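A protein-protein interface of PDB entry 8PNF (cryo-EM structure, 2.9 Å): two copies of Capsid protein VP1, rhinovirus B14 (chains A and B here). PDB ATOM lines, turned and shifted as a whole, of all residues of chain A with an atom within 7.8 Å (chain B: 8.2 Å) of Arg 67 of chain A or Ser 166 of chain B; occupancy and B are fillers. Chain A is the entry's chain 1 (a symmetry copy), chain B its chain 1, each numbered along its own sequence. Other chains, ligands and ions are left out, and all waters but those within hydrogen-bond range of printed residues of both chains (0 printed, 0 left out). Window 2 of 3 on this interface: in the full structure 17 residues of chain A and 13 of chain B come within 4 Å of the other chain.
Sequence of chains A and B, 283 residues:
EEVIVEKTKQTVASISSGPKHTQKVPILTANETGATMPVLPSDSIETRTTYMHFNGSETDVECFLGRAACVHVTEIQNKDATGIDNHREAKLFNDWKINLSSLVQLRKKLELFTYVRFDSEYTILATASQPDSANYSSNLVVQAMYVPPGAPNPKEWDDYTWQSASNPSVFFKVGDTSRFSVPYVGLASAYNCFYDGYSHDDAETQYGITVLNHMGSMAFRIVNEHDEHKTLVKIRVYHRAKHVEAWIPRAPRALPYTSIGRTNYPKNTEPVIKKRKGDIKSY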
ATOM      1  N   GLU A  58     -15.763   9.430  36.993  1.00  0.00           N
ATOM      2  CA  GLU A  58     -16.831   9.910  36.129  1.00  0.00           C
ATOM      3  C   GLU A  58     -16.459   9.847  34.654  1.00  0.00           C
ATOM      4  O   GLU A  58     -17.350   9.864  33.801  1.00  0.00           O
ATOM      5  CB  GLU A  58     -17.209  11.340  36.512  1.00  0.00           C
ATOM      6  CG  GLU A  58     -18.624  11.735  36.129  1.00  0.00           C
ATOM      7  CD  GLU A  58     -19.142  12.896  36.934  1.00  0.00           C
ATOM      8  OE1 GLU A  58     -18.342  13.793  37.258  1.00  0.00           O
ATOM      9  OE2 GLU A  58     -20.350  12.912  37.244  1.00  0.00           O
ATOM     10  N   VAL A  61     -15.935   4.936  30.910  1.00  0.00           N
ATOM     11  CA  VAL A  61     -16.891   4.814  29.814  1.00  0.00           C
ATOM     12  C   VAL A  61     -18.164   4.092  30.219  1.00  0.00           C
ATOM     13  O   VAL A  61     -19.167   4.191  29.508  1.00  0.00           O
ATOM     14  CB  VAL A  61     -16.241   4.118  28.600  1.00  0.00           C
ATOM     15  CG1 VAL A  61     -15.014   4.886  28.151  1.00  0.00           C
ATOM     16  CG2 VAL A  61     -15.882   2.687  28.932  1.00  0.00           C
ATOM     17  N   GLU A  62     -18.146   3.364  31.337  1.00  0.00           N
ATOM     18  CA  GLU A  62     -19.381   2.871  31.928  1.00  0.00           C
ATOM     19  C   GLU A  62     -20.239   4.021  32.436  1.00  0.00           C
ATOM     20  O   GLU A  62     -21.456   4.028  32.238  1.00  0.00           O
ATOM     21  CB  GLU A  62     -19.060   1.895  33.056  1.00  0.00           C
ATOM     22  CG  GLU A  62     -20.271   1.330  33.765  1.00  0.00           C
ATOM     23  CD  GLU A  62     -20.830   0.116  33.070  1.00  0.00           C
ATOM     24  OE1 GLU A  62     -20.040  -0.625  32.455  1.00  0.00           O
ATOM     25  OE2 GLU A  62     -22.056  -0.100  33.146  1.00  0.00           O
ATOM     26  N   CYS A  63     -19.624   5.002  33.092  1.00  0.00           N
ATOM     27  CA  CYS A  63     -20.334   6.194  33.535  1.00  0.00           C
ATOM     28  C   CYS A  63     -20.637   7.152  32.392  1.00  0.00           C
ATOM     29  O   CYS A  63     -21.718   7.755  32.373  1.00  0.00           O
ATOM     30  CB  CYS A  63     -19.513   6.915  34.607  1.00  0.00           C
ATOM     31  SG  CYS A  63     -20.149   8.523  35.130  1.00  0.00           S
ATOM     32  N   PHE A  64     -19.707   7.289  31.440  1.00  0.00           N
ATOM     33  CA  PHE A  64     -19.849   8.243  30.344  1.00  0.00           C
ATOM     34  C   PHE A  64     -21.010   7.898  29.423  1.00  0.00           C
ATOM     35  O   PHE A  64     -21.738   8.794  28.986  1.00  0.00           O
ATOM     36  CB  PHE A  64     -18.542   8.313  29.557  1.00  0.00           C
ATOM     37  CG  PHE A  64     -18.591   9.223  28.368  1.00  0.00           C
ATOM     38  CD1 PHE A  64     -18.829  10.578  28.525  1.00  0.00           C
ATOM     39  CD2 PHE A  64     -18.369   8.729  27.093  1.00  0.00           C
ATOM     40  CE1 PHE A  64     -18.864  11.411  27.438  1.00  0.00           C
ATOM     41  CE2 PHE A  64     -18.401   9.561  26.002  1.00  0.00           C
ATOM     42  CZ  PHE A  64     -18.648  10.907  26.174  1.00  0.00           C
ATOM     43  N   LEU A  65     -21.213   6.617  29.131  1.00  0.00           N
ATOM     44  CA  LEU A  65     -22.293   6.183  28.258  1.00  0.00           C
ATOM     45  C   LEU A  65     -23.470   5.608  29.034  1.00  0.00           C
ATOM     46  O   LEU A  65     -24.447   5.158  28.429  1.00  0.00           O
ATOM     47  CB  LEU A  65     -21.765   5.169  27.244  1.00  0.00           C
ATOM     48  CG  LEU A  65     -20.780   5.778  26.249  1.00  0.00           C
ATOM     49  CD1 LEU A  65     -20.033   4.702  25.489  1.00  0.00           C
ATOM     50  CD2 LEU A  65     -21.517   6.689  25.296  1.00  0.00           C
ATOM     51  N   GLY A  66     -23.413   5.646  30.359  1.00  0.00           N
ATOM     52  CA  GLY A  66     -24.376   4.944  31.180  1.00  0.00           C
ATOM     53  C   GLY A  66     -25.387   5.792  31.919  1.00  0.00           C
ATOM     54  O   GLY A  66     -25.672   5.532  33.090  1.00  0.00           O
ATOM     55  N   ARG A  67     -25.928   6.807  31.258  1.00  0.00           N
ATOM     56  CA  ARG A  67     -27.081   7.525  31.776  1.00  0.00           C
ATOM     57  C   ARG A  67     -28.158   7.531  30.707  1.00  0.00           C
ATOM     58  O   ARG A  67     -27.874   7.406  29.514  1.00  0.00           O
ATOM     59  CB  ARG A  67     -26.722   8.949  32.214  1.00  0.00           C
ATOM     60  CG  ARG A  67     -25.644   9.612  31.385  1.00  0.00           C
ATOM     61  CD  ARG A  67     -25.206  10.906  32.037  1.00  0.00           C
ATOM     62  NE  ARG A  67     -24.597  10.669  33.340  1.00  0.00           N
ATOM     63  CZ  ARG A  67     -24.359  11.618  34.238  1.00  0.00           C
ATOM     64  NH1 ARG A  67     -24.690  12.874  33.984  1.00  0.00           N
ATOM     65  NH2 ARG A  67     -23.802  11.307  35.396  1.00  0.00           N
ATOM     66  N   ALA A  68     -29.407   7.656  31.150  1.00  0.00           N
ATOM     67  CA  ALA A  68     -30.551   7.534  30.257  1.00  0.00           C
ATOM     68  C   ALA A  68     -30.660   8.753  29.352  1.00  0.00           C
ATOM     69  O   ALA A  68     -30.556   9.891  29.813  1.00  0.00           O
ATOM     70  CB  ALA A  68     -31.835   7.345  31.059  1.00  0.00           C
ATOM     71  N   ALA A  69     -30.839   8.506  28.058  1.00  0.00           N
ATOM     72  CA  ALA A  69     -30.954   9.548  27.051  1.00  0.00           C
ATOM     73  C   ALA A  69     -32.116   9.226  26.124  1.00  0.00           C
ATOM     74  O   ALA A  69     -32.382   8.057  25.838  1.00  0.00           O
ATOM     75  CB  ALA A  69     -29.663   9.681  26.247  1.00  0.00           C
ATOM     76  N   CYS A  70     -32.796  10.263  25.647  1.00  0.00           N
ATOM     77  CA  CYS A  70     -34.000  10.090  24.835  1.00  0.00           C
ATOM     78  C   CYS A  70     -33.600   9.698  23.421  1.00  0.00           C
ATOM     79  O   CYS A  70     -33.019  10.493  22.688  1.00  0.00           O
ATOM     80  CB  CYS A  70     -34.826  11.370  24.833  1.00  0.00           C
ATOM     81  SG  CYS A  70     -36.426  11.235  24.013  1.00  0.00           S
ATOM     82  N   GLN A 105     -27.047  13.954  20.413  1.00  0.00           N
ATOM     83  CA  GLN A 105     -26.254  14.091  21.635  1.00  0.00           C
ATOM     84  C   GLN A 105     -25.733  12.755  22.150  1.00  0.00           C
ATOM     85  O   GLN A 105     -24.560  12.658  22.521  1.00  0.00           O
ATOM     86  CB  GLN A 105     -27.067  14.786  22.725  1.00  0.00           C
ATOM     87  CG  GLN A 105     -27.120  16.308  22.623  1.00  0.00           C
ATOM     88  CD  GLN A 105     -25.785  16.981  22.926  1.00  0.00           C
ATOM     89  OE1 GLN A 105     -25.007  16.501  23.749  1.00  0.00           O
ATOM     90  NE2 GLN A 105     -25.516  18.092  22.254  1.00  0.00           N
ATOM     91  N   LEU A 106     -26.575  11.724  22.192  1.00  0.00           N
ATOM     92  CA  LEU A 106     -26.076  10.390  22.501  1.00  0.00           C
ATOM     93  C   LEU A 106     -25.218   9.836  21.376  1.00  0.00           C
ATOM     94  O   LEU A 106     -24.263   9.096  21.642  1.00  0.00           O
ATOM     95  CB  LEU A 106     -27.239   9.435  22.791  1.00  0.00           C
ATOM     96  CG  LEU A 106     -26.923   7.966  23.119  1.00  0.00           C
ATOM     97  CD1 LEU A 106     -25.917   7.853  24.245  1.00  0.00           C
ATOM     98  CD2 LEU A 106     -28.173   7.207  23.470  1.00  0.00           C
ATOM     99  N   LYS A 109     -21.596  10.866  21.648  1.00  0.00           N
ATOM    100  CA  LYS A 109     -20.924  10.157  22.731  1.00  0.00           C
ATOM    101  C   LYS A 109     -20.643   8.713  22.343  1.00  0.00           C
ATOM    102  O   LYS A 109     -19.627   8.139  22.750  1.00  0.00           O
ATOM    103  CB  LYS A 109     -21.767  10.220  24.001  1.00  0.00           C
ATOM    104  CG  LYS A 109     -22.027  11.626  24.499  1.00  0.00           C
ATOM    105  CD  LYS A 109     -22.193  11.694  26.010  1.00  0.00           C
ATOM    106  CE  LYS A 109     -23.132  10.632  26.537  1.00  0.00           C
ATOM    107  NZ  LYS A 109     -23.070  10.550  28.016  1.00  0.00           N
ATOM    108  N   GLU A 121     -30.809  -0.746  28.668  1.00  0.00           N
ATOM    109  CA  GLU A 121     -31.878  -0.514  29.630  1.00  0.00           C
ATOM    110  C   GLU A 121     -32.824   0.507  29.018  1.00  0.00           C
ATOM    111  O   GLU A 121     -32.440   1.660  28.805  1.00  0.00           O
ATOM    112  CB  GLU A 121     -31.323  -0.012  30.958  1.00  0.00           C
ATOM    113  CG  GLU A 121     -32.360   0.179  32.040  1.00  0.00           C
ATOM    114  CD  GLU A 121     -31.741   0.636  33.345  1.00  0.00           C
ATOM    115  OE1 GLU A 121     -30.508   0.821  33.388  1.00  0.00           O
ATOM    116  OE2 GLU A 121     -32.474   0.804  34.334  1.00  0.00           O
ATOM    117  N   TYR A 238     -36.283   6.096  26.382  1.00  0.00           N
ATOM    118  CA  TYR A 238     -35.018   6.456  26.998  1.00  0.00           C
ATOM    119  C   TYR A 238     -34.124   5.229  27.096  1.00  0.00           C
ATOM    120  O   TYR A 238     -34.549   4.182  27.587  1.00  0.00           O
ATOM    121  CB  TYR A 238     -35.237   7.065  28.386  1.00  0.00           C
ATOM    122  CG  TYR A 238     -35.816   8.454  28.332  1.00  0.00           C
ATOM    123  CD1 TYR A 238     -37.184   8.655  28.218  1.00  0.00           C
ATOM    124  CD2 TYR A 238     -34.993   9.567  28.380  1.00  0.00           C
ATOM    125  CE1 TYR A 238     -37.714   9.922  28.157  1.00  0.00           C
ATOM    126  CE2 TYR A 238     -35.517  10.838  28.320  1.00  0.00           C
ATOM    127  CZ  TYR A 238     -36.876  11.008  28.206  1.00  0.00           C
ATOM    128  OH  TYR A 238     -37.401  12.276  28.145  1.00  0.00           O
ATOM    129  N   HIS A 239     -32.886   5.367  26.634  1.00  0.00           N
ATOM    130  CA  HIS A 239     -31.928   4.271  26.625  1.00  0.00           C
ATOM    131  C   HIS A 239     -30.798   4.580  27.590  1.00  0.00           C
ATOM    132  O   HIS A 239     -30.221   5.668  27.546  1.00  0.00           O
ATOM    133  CB  HIS A 239     -31.368   4.035  25.218  1.00  0.00           C
ATOM    134  CG  HIS A 239     -30.336   2.952  25.146  1.00  0.00           C
ATOM    135  ND1 HIS A 239     -29.000   3.178  25.394  1.00  0.00           N
ATOM    136  CD2 HIS A 239     -30.444   1.637  24.844  1.00  0.00           C
ATOM    137  CE1 HIS A 239     -28.331   2.049  25.264  1.00  0.00           C
ATOM    138  NE2 HIS A 239     -29.182   1.100  24.920  1.00  0.00           N
ATOM    139  N   ARG A 240     -30.479   3.618  28.447  1.00  0.00           N
ATOM    140  CA  ARG A 240     -29.292   3.665  29.291  1.00  0.00           C
ATOM    141  C   ARG A 240     -28.441   2.446  28.968  1.00  0.00           C
ATOM    142  O   ARG A 240     -28.929   1.314  29.015  1.00  0.00           O
ATOM    143  CB  ARG A 240     -29.661   3.696  30.772  1.00  0.00           C
ATOM    144  CG  ARG A 240     -28.465   3.614  31.690  1.00  0.00           C
ATOM    145  CD  ARG A 240     -28.840   3.834  33.134  1.00  0.00           C
ATOM    146  NE  ARG A 240     -28.852   2.584  33.882  1.00  0.00           N
ATOM    147  CZ  ARG A 240     -27.783   2.036  34.445  1.00  0.00           C
ATOM    148  NH1 ARG A 240     -26.602   2.628  34.353  1.00  0.00           N
ATOM    149  NH2 ARG A 240     -27.897   0.895  35.103  1.00  0.00           N
ATOM    150  N   ALA A 241     -27.180   2.677  28.623  1.00  0.00           N
ATOM    151  CA  ALA A 241     -26.247   1.586  28.392  1.00  0.00           C
ATOM    152  C   ALA A 241     -25.659   1.136  29.719  1.00  0.00           C
ATOM    153  O   ALA A 241     -25.511   1.936  30.643  1.00  0.00           O
ATOM    154  CB  ALA A 241     -25.132   2.014  27.442  1.00  0.00           C
ATOM    155  N   LYS A 242     -25.337  -0.144  29.821  1.00  0.00           N
ATOM    156  CA  LYS A 242     -24.649  -0.664  30.989  1.00  0.00           C
ATOM    157  C   LYS A 242     -23.803  -1.853  30.576  1.00  0.00           C
ATOM    158  O   LYS A 242     -24.041  -2.465  29.533  1.00  0.00           O
ATOM    159  CB  LYS A 242     -25.620  -1.064  32.103  1.00  0.00           C
ATOM    160  CG  LYS A 242     -26.942  -1.616  31.639  1.00  0.00           C
ATOM    161  CD  LYS A 242     -27.756  -2.021  32.841  1.00  0.00           C
ATOM    162  CE  LYS A 242     -29.052  -2.687  32.456  1.00  0.00           C
ATOM    163  NZ  LYS A 242     -29.814  -3.051  33.675  1.00  0.00           N
ATOM    164  N   VAL A 244     -20.694  -1.567  29.742  1.00  0.00           N
ATOM    165  CA  VAL A 244     -20.208  -1.008  28.488  1.00  0.00           C
ATOM    166  C   VAL A 244     -18.758  -1.405  28.276  1.00  0.00           C
ATOM    167  O   VAL A 244     -17.929  -1.300  29.185  1.00  0.00           O
ATOM    168  CB  VAL A 244     -20.354   0.522  28.482  1.00  0.00           C
ATOM    169  CG1 VAL A 244     -20.137   1.074  27.086  1.00  0.00           C
ATOM    170  CG2 VAL A 244     -21.693   0.936  29.022  1.00  0.00           C
ATOM    171  N   MET B 145     -34.487  19.806  35.034  1.00  0.00           N
ATOM    172  CA  MET B 145     -33.183  19.448  34.497  1.00  0.00           C
ATOM    173  C   MET B 145     -32.103  20.269  35.189  1.00  0.00           C
ATOM    174  O   MET B 145     -32.138  21.500  35.147  1.00  0.00           O
ATOM    175  CB  MET B 145     -33.137  19.687  32.991  1.00  0.00           C
ATOM    176  CG  MET B 145     -31.788  19.419  32.377  1.00  0.00           C
ATOM    177  SD  MET B 145     -31.812  19.375  30.581  1.00  0.00           S
ATOM    178  CE  MET B 145     -32.314  21.041  30.193  1.00  0.00           C
ATOM    179  N   TYR B 146     -31.135  19.591  35.795  1.00  0.00           N
ATOM    180  CA  TYR B 146     -30.032  20.280  36.454  1.00  0.00           C
ATOM    181  C   TYR B 146     -29.000  20.696  35.414  1.00  0.00           C
ATOM    182  O   TYR B 146     -28.344  19.848  34.807  1.00  0.00           O
ATOM    183  CB  TYR B 146     -29.411  19.371  37.510  1.00  0.00           C
ATOM    184  CG  TYR B 146     -28.208  19.938  38.221  1.00  0.00           C
ATOM    185  CD1 TYR B 146     -28.350  20.900  39.213  1.00  0.00           C
ATOM    186  CD2 TYR B 146     -26.930  19.486  37.925  1.00  0.00           C
ATOM    187  CE1 TYR B 146     -27.252  21.409  39.873  1.00  0.00           C
ATOM    188  CE2 TYR B 146     -25.829  19.988  38.581  1.00  0.00           C
ATOM    189  CZ  TYR B 146     -25.995  20.948  39.553  1.00  0.00           C
ATOM    190  OH  TYR B 146     -24.898  21.447  40.208  1.00  0.00           O
ATOM    191  N   PRO B 148     -25.620  22.501  34.529  1.00  0.00           N
ATOM    192  CA  PRO B 148     -24.358  23.043  35.051  1.00  0.00           C
ATOM    193  C   PRO B 148     -23.938  24.284  34.283  1.00  0.00           C
ATOM    194  O   PRO B 148     -24.478  24.557  33.202  1.00  0.00           O
ATOM    195  CB  PRO B 148     -23.367  21.886  34.835  1.00  0.00           C
ATOM    196  CG  PRO B 148     -24.217  20.681  34.606  1.00  0.00           C
ATOM    197  CD  PRO B 148     -25.428  21.182  33.909  1.00  0.00           C
ATOM    198  N   ALA B 151     -23.213  24.564  30.166  1.00  0.00           N
ATOM    199  CA  ALA B 151     -24.139  23.746  29.403  1.00  0.00           C
ATOM    200  C   ALA B 151     -25.038  24.637  28.543  1.00  0.00           C
ATOM    201  O   ALA B 151     -25.224  25.817  28.851  1.00  0.00           O
ATOM    202  CB  ALA B 151     -24.980  22.893  30.349  1.00  0.00           C
ATOM    203  N   THR B 161     -32.266  20.826  24.093  1.00  0.00           N
ATOM    204  CA  THR B 161     -31.484  20.673  25.315  1.00  0.00           C
ATOM    205  C   THR B 161     -32.190  19.848  26.378  1.00  0.00           C
ATOM    206  O   THR B 161     -31.534  19.381  27.313  1.00  0.00           O
ATOM    207  CB  THR B 161     -31.126  22.038  25.896  1.00  0.00           C
ATOM    208  OG1 THR B 161     -32.298  22.632  26.459  1.00  0.00           O
ATOM    209  CG2 THR B 161     -30.523  22.939  24.846  1.00  0.00           C
ATOM    210  N   GLN B 163     -33.347  16.898  26.196  1.00  0.00           N
ATOM    211  CA  GLN B 163     -33.104  15.465  26.098  1.00  0.00           C
ATOM    212  C   GLN B 163     -32.099  14.970  27.127  1.00  0.00           C
ATOM    213  O   GLN B 163     -32.242  13.839  27.601  1.00  0.00           O
ATOM    214  CB  GLN B 163     -32.640  15.101  24.688  1.00  0.00           C
ATOM    215  CG  GLN B 163     -33.369  15.840  23.571  1.00  0.00           C
ATOM    216  CD  GLN B 163     -34.883  15.762  23.679  1.00  0.00           C
ATOM    217  OE1 GLN B 163     -35.469  14.681  23.630  1.00  0.00           O
ATOM    218  NE2 GLN B 163     -35.523  16.918  23.817  1.00  0.00           N
ATOM    219  N   SER B 164     -31.105  15.796  27.473  1.00  0.00           N
ATOM    220  CA  SER B 164     -30.243  15.653  28.653  1.00  0.00           C
ATOM    221  C   SER B 164     -29.487  14.324  28.670  1.00  0.00           C
ATOM    222  O   SER B 164     -29.687  13.474  29.539  1.00  0.00           O
ATOM    223  CB  SER B 164     -31.037  15.836  29.953  1.00  0.00           C
ATOM    224  OG  SER B 164     -31.927  14.761  30.190  1.00  0.00           O
ATOM    225  N   ALA B 165     -28.613  14.153  27.681  1.00  0.00           N
ATOM    226  CA  ALA B 165     -27.760  12.978  27.657  1.00  0.00           C
ATOM    227  C   ALA B 165     -26.670  13.033  28.717  1.00  0.00           C
ATOM    228  O   ALA B 165     -26.191  11.981  29.151  1.00  0.00           O
ATOM    229  CB  ALA B 165     -27.138  12.806  26.274  1.00  0.00           C
ATOM    230  N   SER B 166     -26.275  14.229  29.150  1.00  0.00           N
ATOM    231  CA  SER B 166     -25.248  14.367  30.171  1.00  0.00           C
ATOM    232  C   SER B 166     -25.794  15.061  31.412  1.00  0.00           C
ATOM    233  O   SER B 166     -25.413  14.714  32.533  1.00  0.00           O
ATOM    234  CB  SER B 166     -24.050  15.136  29.620  1.00  0.00           C
ATOM    235  OG  SER B 166     -23.443  14.432  28.556  1.00  0.00           O
ATOM    236  N   ASN B 167     -26.666  16.046  31.220  1.00  0.00           N
ATOM    237  CA  ASN B 167     -27.252  16.770  32.345  1.00  0.00           C
ATOM    238  C   ASN B 167     -28.211  15.868  33.113  1.00  0.00           C
ATOM    239  O   ASN B 167     -29.021  15.172  32.496  1.00  0.00           O
ATOM    240  CB  ASN B 167     -28.001  18.011  31.869  1.00  0.00           C
ATOM    241  CG  ASN B 167     -27.104  19.010  31.180  1.00  0.00           C
ATOM    242  OD1 ASN B 167     -25.890  19.002  31.362  1.00  0.00           O
ATOM    243  ND2 ASN B 167     -27.703  19.896  30.402  1.00  0.00           N
ATOM    244  N   PRO B 168     -28.144  15.839  34.444  1.00  0.00           N
ATOM    245  CA  PRO B 168     -29.116  15.047  35.210  1.00  0.00           C
ATOM    246  C   PRO B 168     -30.476  15.731  35.254  1.00  0.00           C
ATOM    247  O   PRO B 168     -30.577  16.930  35.516  1.00  0.00           O
ATOM    248  CB  PRO B 168     -28.480  14.961  36.602  1.00  0.00           C
ATOM    249  CG  PRO B 168     -27.583  16.124  36.675  1.00  0.00           C
ATOM    250  CD  PRO B 168     -27.066  16.358  35.298  1.00  0.00           C
ATOM    251  N   SER B 169     -31.523  14.953  34.998  1.00  0.00           N
ATOM    252  CA  SER B 169     -32.889  15.446  35.029  1.00  0.00           C
ATOM    253  C   SER B 169     -33.779  14.448  35.754  1.00  0.00           C
ATOM    254  O   SER B 169     -33.460  13.264  35.867  1.00  0.00           O
ATOM    255  CB  SER B 169     -33.431  15.709  33.620  1.00  0.00           C
ATOM    256  OG  SER B 169     -33.318  14.555  32.813  1.00  0.00           O
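The side-chain amide oxygen of Gln 163 of chain B sits close to the side-chain sulfur of Cys 70 of chain A, at 3.6 Å. NH1 of Arg 67 of chain A lies within hydrogen-bond range of O of Ser 166 of chain B, 2.5 Å away.
OG of Ser 164 of chain B sits at hydrogen-bond distance from OG of Ser 169 of chain B, at 3.0 Å. The backbone carbonyl oxygen (O) of Phe 64 of chain A lies within hydrogen-bond range of the side-chain amino group (NZ) of Lys 109 of chain A (2.4 Å).
Among the printed residues, merely in contact across the chains: Arg 67 of chain A with Ala 165 of chain B (3.2 Å), Lys 109 of chain A with Ala 165 of chain B (3.6 Å), Ala 68 of chain A with Ser 164 of chain B (3.7 Å) and Lys 109 of chain A with Ser 166 of chain B (3.9 Å).
No residue of chain B comes within 4 Å of Gly 66 of chain A. Of the printed residues of chain B, Cys 70 of chain A touches Gln 163. Of the printed residues of chain B, Lys 109 of chain A touches Ala 165 (3.6 Å) and Ser 166 (3.9 Å). Thr 161 of chain B touches none of the printed residues of chain A. Of the printed residues of chain A, Gln 163 of chain B touches Cys 70. Of the printed residues of chain A, Ser 164 of chain B touches Ala 68 (3.7 Å). Printed residues of chain A within 4 Å of Ala 165 of chain B: Arg 67 (3.2 Å) and Lys 109 (3.6 Å). The nearest residue of chain A that does not touch Ser 166 of chain B is Gln 105 of chain A (5.5 Å).
Of the 12 printed residues of chain B, 4 touch a printed residue of chain A. Of the 21 printed residues of chain A, 4 touch a printed residue of chain B. Among the printed residues, no Asp or Glu carboxylate lies within 4 Å of a Lys or Arg side-chain nitrogen of the other chain.
No position is printed for both chains. Of the 6 pairs that touch across the chains among the printed residues, none has its exchanged pair printed and touching as well.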
